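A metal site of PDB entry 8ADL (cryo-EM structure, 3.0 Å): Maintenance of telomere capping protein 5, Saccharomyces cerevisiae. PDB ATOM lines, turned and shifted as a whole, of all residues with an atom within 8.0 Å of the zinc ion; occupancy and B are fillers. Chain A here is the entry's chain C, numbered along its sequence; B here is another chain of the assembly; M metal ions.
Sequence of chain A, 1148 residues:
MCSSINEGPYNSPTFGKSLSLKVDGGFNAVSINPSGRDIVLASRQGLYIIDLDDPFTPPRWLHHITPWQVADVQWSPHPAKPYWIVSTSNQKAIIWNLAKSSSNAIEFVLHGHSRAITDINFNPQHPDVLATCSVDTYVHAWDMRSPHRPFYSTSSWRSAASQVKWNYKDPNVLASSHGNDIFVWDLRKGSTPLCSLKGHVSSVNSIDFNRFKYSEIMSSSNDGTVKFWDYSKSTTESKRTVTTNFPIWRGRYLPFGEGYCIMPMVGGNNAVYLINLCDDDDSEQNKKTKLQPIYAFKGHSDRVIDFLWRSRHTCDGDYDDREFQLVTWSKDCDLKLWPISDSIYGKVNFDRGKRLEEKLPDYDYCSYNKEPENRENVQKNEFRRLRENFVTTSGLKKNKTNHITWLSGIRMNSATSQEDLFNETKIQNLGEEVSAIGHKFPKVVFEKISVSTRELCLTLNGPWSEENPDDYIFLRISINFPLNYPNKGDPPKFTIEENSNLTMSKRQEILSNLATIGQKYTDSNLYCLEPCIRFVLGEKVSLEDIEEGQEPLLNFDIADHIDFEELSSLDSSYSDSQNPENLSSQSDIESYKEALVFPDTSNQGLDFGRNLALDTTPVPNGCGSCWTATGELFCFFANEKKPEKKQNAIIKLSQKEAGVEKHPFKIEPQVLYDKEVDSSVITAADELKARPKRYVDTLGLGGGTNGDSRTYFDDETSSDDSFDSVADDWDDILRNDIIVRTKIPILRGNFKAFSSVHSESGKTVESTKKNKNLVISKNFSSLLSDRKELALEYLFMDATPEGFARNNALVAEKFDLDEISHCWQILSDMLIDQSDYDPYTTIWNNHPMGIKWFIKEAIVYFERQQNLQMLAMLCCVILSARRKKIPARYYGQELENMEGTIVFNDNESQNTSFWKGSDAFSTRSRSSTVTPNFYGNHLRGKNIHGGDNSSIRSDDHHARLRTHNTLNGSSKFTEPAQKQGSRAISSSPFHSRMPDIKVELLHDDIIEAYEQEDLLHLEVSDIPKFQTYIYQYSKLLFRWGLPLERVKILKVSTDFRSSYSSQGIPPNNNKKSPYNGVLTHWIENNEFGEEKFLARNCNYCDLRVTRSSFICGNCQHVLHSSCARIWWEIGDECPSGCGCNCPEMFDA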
ATOM      1  N   ASN A1097      -9.876   1.700 -26.293  1.00  0.00           N
ATOM      2  CA  ASN A1097     -10.638   2.747 -25.617  1.00  0.00           C
ATOM      3  C   ASN A1097     -10.363   2.731 -24.120  1.00  0.00           C
ATOM      4  O   ASN A1097     -10.208   1.661 -23.526  1.00  0.00           O
ATOM      5  CB  ASN A1097     -12.148   2.608 -25.861  1.00  0.00           C
ATOM      6  CG  ASN A1097     -12.592   3.225 -27.174  1.00  0.00           C
ATOM      7  OD1 ASN A1097     -12.054   4.229 -27.607  1.00  0.00           O
ATOM      8  ND2 ASN A1097     -13.591   2.620 -27.804  1.00  0.00           N
ATOM      9  N   CYS A1098     -10.303   3.915 -23.532  1.00  0.00           N
ATOM     10  CA  CYS A1098     -10.103   4.045 -22.094  1.00  0.00           C
ATOM     11  C   CYS A1098     -11.288   3.466 -21.329  1.00  0.00           C
ATOM     12  O   CYS A1098     -12.428   3.508 -21.782  1.00  0.00           O
ATOM     13  CB  CYS A1098      -9.907   5.522 -21.728  1.00  0.00           C
ATOM     14  SG  CYS A1098      -9.771   5.870 -19.960  1.00  0.00           S
ATOM     15  N   ASN A1099     -10.995   2.914 -20.153  1.00  0.00           N
ATOM     16  CA  ASN A1099     -12.006   2.249 -19.346  1.00  0.00           C
ATOM     17  C   ASN A1099     -12.696   3.175 -18.353  1.00  0.00           C
ATOM     18  O   ASN A1099     -13.538   2.722 -17.578  1.00  0.00           O
ATOM     19  CB  ASN A1099     -11.378   1.070 -18.597  1.00  0.00           C
ATOM     20  CG  ASN A1099     -11.018  -0.071 -19.528  1.00  0.00           C
ATOM     21  OD1 ASN A1099     -11.870  -0.889 -19.875  1.00  0.00           O
ATOM     22  ND2 ASN A1099      -9.760  -0.119 -19.942  1.00  0.00           N
ATOM     23  N   TYR A1100     -12.354   4.461 -18.357  1.00  0.00           N
ATOM     24  CA  TYR A1100     -12.998   5.470 -17.532  1.00  0.00           C
ATOM     25  C   TYR A1100     -13.883   6.416 -18.305  1.00  0.00           C
ATOM     26  O   TYR A1100     -14.967   6.785 -17.827  1.00  0.00           O
ATOM     27  CB  TYR A1100     -11.934   6.276 -16.770  1.00  0.00           C
ATOM     28  CG  TYR A1100     -12.478   7.193 -15.706  1.00  0.00           C
ATOM     29  CD1 TYR A1100     -12.840   6.694 -14.457  1.00  0.00           C
ATOM     30  CD2 TYR A1100     -12.620   8.551 -15.928  1.00  0.00           C
ATOM     31  CE1 TYR A1100     -13.329   7.527 -13.475  1.00  0.00           C
ATOM     32  CE2 TYR A1100     -13.108   9.395 -14.954  1.00  0.00           C
ATOM     33  CZ  TYR A1100     -13.460   8.874 -13.722  1.00  0.00           C
ATOM     34  OH  TYR A1100     -13.953   9.714 -12.756  1.00  0.00           O
ATOM     35  N   CYS A1101     -13.470   6.825 -19.505  1.00  0.00           N
ATOM     36  CA  CYS A1101     -14.189   7.803 -20.303  1.00  0.00           C
ATOM     37  C   CYS A1101     -14.697   7.266 -21.636  1.00  0.00           C
ATOM     38  O   CYS A1101     -15.455   7.964 -22.305  1.00  0.00           O
ATOM     39  CB  CYS A1101     -13.312   9.037 -20.567  1.00  0.00           C
ATOM     40  SG  CYS A1101     -11.844   8.680 -21.550  1.00  0.00           S
ATOM     41  N   ASP A1102     -14.284   6.050 -22.028  1.00  0.00           N
ATOM     42  CA  ASP A1102     -14.645   5.412 -23.293  1.00  0.00           C
ATOM     43  C   ASP A1102     -14.272   6.279 -24.499  1.00  0.00           C
ATOM     44  O   ASP A1102     -15.002   6.372 -25.487  1.00  0.00           O
ATOM     45  CB  ASP A1102     -16.126   5.036 -23.344  1.00  0.00           C
ATOM     46  CG  ASP A1102     -16.434   3.795 -22.522  1.00  0.00           C
ATOM     47  OD1 ASP A1102     -15.546   2.923 -22.416  1.00  0.00           O
ATOM     48  OD2 ASP A1102     -17.562   3.691 -21.993  1.00  0.00           O
ATOM     49  N   LEU A1103     -13.106   6.923 -24.415  1.00  0.00           N
ATOM     50  CA  LEU A1103     -12.494   7.628 -25.522  1.00  0.00           C
ATOM     51  C   LEU A1103     -11.245   6.880 -25.960  1.00  0.00           C
ATOM     52  O   LEU A1103     -10.692   6.056 -25.218  1.00  0.00           O
ATOM     53  CB  LEU A1103     -12.132   9.068 -25.143  1.00  0.00           C
ATOM     54  CG  LEU A1103     -13.264   9.999 -24.699  1.00  0.00           C
ATOM     55  CD1 LEU A1103     -12.711  11.312 -24.192  1.00  0.00           C
ATOM     56  CD2 LEU A1103     -14.242  10.235 -25.835  1.00  0.00           C
ATOM     57  N   ARG A1104     -10.802   7.150 -27.188  1.00  0.00           N
ATOM     58  CA  ARG A1104      -9.629   6.461 -27.720  1.00  0.00           C
ATOM     59  C   ARG A1104      -8.366   6.955 -27.014  1.00  0.00           C
ATOM     60  O   ARG A1104      -8.138   8.157 -26.904  1.00  0.00           O
ATOM     61  CB  ARG A1104      -9.506   6.694 -29.224  1.00  0.00           C
ATOM     62  CG  ARG A1104      -8.416   5.858 -29.875  1.00  0.00           C
ATOM     63  CD  ARG A1104      -8.326   6.120 -31.367  1.00  0.00           C
ATOM     64  NE  ARG A1104      -7.215   5.390 -31.970  1.00  0.00           N
ATOM     65  CZ  ARG A1104      -6.874   5.476 -33.251  1.00  0.00           C
ATOM     66  NH1 ARG A1104      -7.531   6.258 -34.093  1.00  0.00           N
ATOM     67  NH2 ARG A1104      -5.844   4.763 -33.696  1.00  0.00           N
ATOM     68  N   VAL A1105      -7.560   6.012 -26.537  1.00  0.00           N
ATOM     69  CA  VAL A1105      -6.304   6.325 -25.861  1.00  0.00           C
ATOM     70  C   VAL A1105      -5.150   6.202 -26.842  1.00  0.00           C
ATOM     71  O   VAL A1105      -5.063   5.239 -27.619  1.00  0.00           O
ATOM     72  CB  VAL A1105      -6.113   5.460 -24.592  1.00  0.00           C
ATOM     73  CG1 VAL A1105      -5.977   3.969 -24.912  1.00  0.00           C
ATOM     74  CG2 VAL A1105      -4.911   5.942 -23.801  1.00  0.00           C
ATOM     75  N   VAL A1118      -6.447  -0.446 -20.363  1.00  0.00           N
ATOM     76  CA  VAL A1118      -5.821   0.869 -20.457  1.00  0.00           C
ATOM     77  C   VAL A1118      -6.612   1.881 -19.630  1.00  0.00           C
ATOM     78  O   VAL A1118      -7.795   1.686 -19.331  1.00  0.00           O
ATOM     79  CB  VAL A1118      -5.715   1.335 -21.914  1.00  0.00           C
ATOM     80  CG1 VAL A1118      -4.724   0.498 -22.669  1.00  0.00           C
ATOM     81  CG2 VAL A1118      -7.071   1.282 -22.582  1.00  0.00           C
ATOM     82  N   LEU A1119      -5.949   2.980 -19.279  1.00  0.00           N
ATOM     83  CA  LEU A1119      -6.579   4.185 -18.780  1.00  0.00           C
ATOM     84  C   LEU A1119      -5.761   5.374 -19.237  1.00  0.00           C
ATOM     85  O   LEU A1119      -4.547   5.270 -19.436  1.00  0.00           O
ATOM     86  CB  LEU A1119      -6.682   4.196 -17.244  1.00  0.00           C
ATOM     87  CG  LEU A1119      -7.736   3.356 -16.532  1.00  0.00           C
ATOM     88  CD1 LEU A1119      -7.650   3.555 -15.037  1.00  0.00           C
ATOM     89  CD2 LEU A1119      -9.121   3.711 -17.039  1.00  0.00           C
ATOM     90  N   HIS A1120      -6.426   6.520 -19.410  1.00  0.00           N
ATOM     91  CA  HIS A1120      -5.685   7.769 -19.606  1.00  0.00           C
ATOM     92  C   HIS A1120      -4.977   8.151 -18.320  1.00  0.00           C
ATOM     93  O   HIS A1120      -5.335   7.707 -17.221  1.00  0.00           O
ATOM     94  CB  HIS A1120      -6.632   8.884 -20.042  1.00  0.00           C
ATOM     95  CG  HIS A1120      -7.094   8.775 -21.463  1.00  0.00           C
ATOM     96  ND1 HIS A1120      -8.407   8.510 -21.787  1.00  0.00           N
ATOM     97  CD2 HIS A1120      -6.436   8.917 -22.630  1.00  0.00           C
ATOM     98  CE1 HIS A1120      -8.529   8.485 -23.100  1.00  0.00           C
ATOM     99  NE2 HIS A1120      -7.348   8.718 -23.643  1.00  0.00           N
ATOM    100  N   SER A1121      -3.941   8.989 -18.449  1.00  0.00           N
ATOM    101  CA  SER A1121      -3.221   9.469 -17.266  1.00  0.00           C
ATOM    102  C   SER A1121      -4.122  10.341 -16.398  1.00  0.00           C
ATOM    103  O   SER A1121      -4.122  10.197 -15.165  1.00  0.00           O
ATOM    104  CB  SER A1121      -1.978  10.236 -17.683  1.00  0.00           C
ATOM    105  OG  SER A1121      -1.081  10.378 -16.593  1.00  0.00           O
ATOM    106  N   SER A1122      -4.889  11.239 -17.014  1.00  0.00           N
ATOM    107  CA  SER A1122      -5.849  12.048 -16.257  1.00  0.00           C
ATOM    108  C   SER A1122      -6.970  11.182 -15.691  1.00  0.00           C
ATOM    109  O   SER A1122      -7.383  11.381 -14.544  1.00  0.00           O
ATOM    110  CB  SER A1122      -6.408  13.154 -17.143  1.00  0.00           C
ATOM    111  OG  SER A1122      -5.386  14.049 -17.550  1.00  0.00           O
ATOM    112  N   CYS A1123      -7.451  10.215 -16.474  1.00  0.00           N
ATOM    113  CA  CYS A1123      -8.508   9.335 -16.003  1.00  0.00           C
ATOM    114  C   CYS A1123      -8.024   8.445 -14.860  1.00  0.00           C
ATOM    115  O   CYS A1123      -8.775   8.201 -13.907  1.00  0.00           O
ATOM    116  CB  CYS A1123      -9.020   8.479 -17.161  1.00  0.00           C
ATOM    117  SG  CYS A1123      -9.852   9.422 -18.452  1.00  0.00           S
ATOM    118  N   ALA A1124      -6.781   7.973 -14.921  1.00  0.00           N
ATOM    119  CA  ALA A1124      -6.232   7.188 -13.822  1.00  0.00           C
ATOM    120  C   ALA A1124      -6.020   8.050 -12.589  1.00  0.00           C
ATOM    121  O   ALA A1124      -6.335   7.618 -11.470  1.00  0.00           O
ATOM    122  CB  ALA A1124      -4.927   6.515 -14.238  1.00  0.00           C
ATOM    123  N   PHE B 847     -18.612  10.238 -15.543  1.00  0.00           N
ATOM    124  CA  PHE B 847     -17.796   9.053 -15.729  1.00  0.00           C
ATOM    125  C   PHE B 847     -17.494   8.351 -14.410  1.00  0.00           C
ATOM    126  O   PHE B 847     -17.399   7.116 -14.371  1.00  0.00           O
ATOM    127  CB  PHE B 847     -16.491   9.430 -16.434  1.00  0.00           C
ATOM    128  CG  PHE B 847     -16.687  10.036 -17.788  1.00  0.00           C
ATOM    129  CD1 PHE B 847     -17.308   9.314 -18.800  1.00  0.00           C
ATOM    130  CD2 PHE B 847     -16.254  11.326 -18.051  1.00  0.00           C
ATOM    131  CE1 PHE B 847     -17.483   9.873 -20.051  1.00  0.00           C
ATOM    132  CE2 PHE B 847     -16.435  11.892 -19.303  1.00  0.00           C
ATOM    133  CZ  PHE B 847     -17.058  11.159 -20.307  1.00  0.00           C
HETATM  134 ZN    ZN M   1      -9.912   8.144 -20.389  1.00  0.00          ZN
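NE2 of His 1120 is in hydrogen-bond range of O of Arg 1104 (3.4 Å). SG of Cys 1101 sits close to N of Leu 1103 (3.6 Å). The side-chain sulfur (SG) of Cys 1098 sits close to the backbone NH (N) of Tyr 1100 (3.4 Å). The backbone carbonyl oxygen of Leu 1103 sits at hydrogen-bond distance from the backbone NH of Cys 1098, at 2.8 Å.
Four residues have an atom within 4 Å of the zinc ion: Cys 1098, Cys 1101, His 1120 and Cys 1123. The nearest printed residue that does not touch the zinc ion is Tyr 1100 (4.5 Å).
The zinc ion is bound by ND1 of His 1120 (2.1 Å), SG of Cys 1101 (2.3 Å), SG of Cys 1098 (2.3 Å) and SG of Cys 1123 (2.3 Å).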
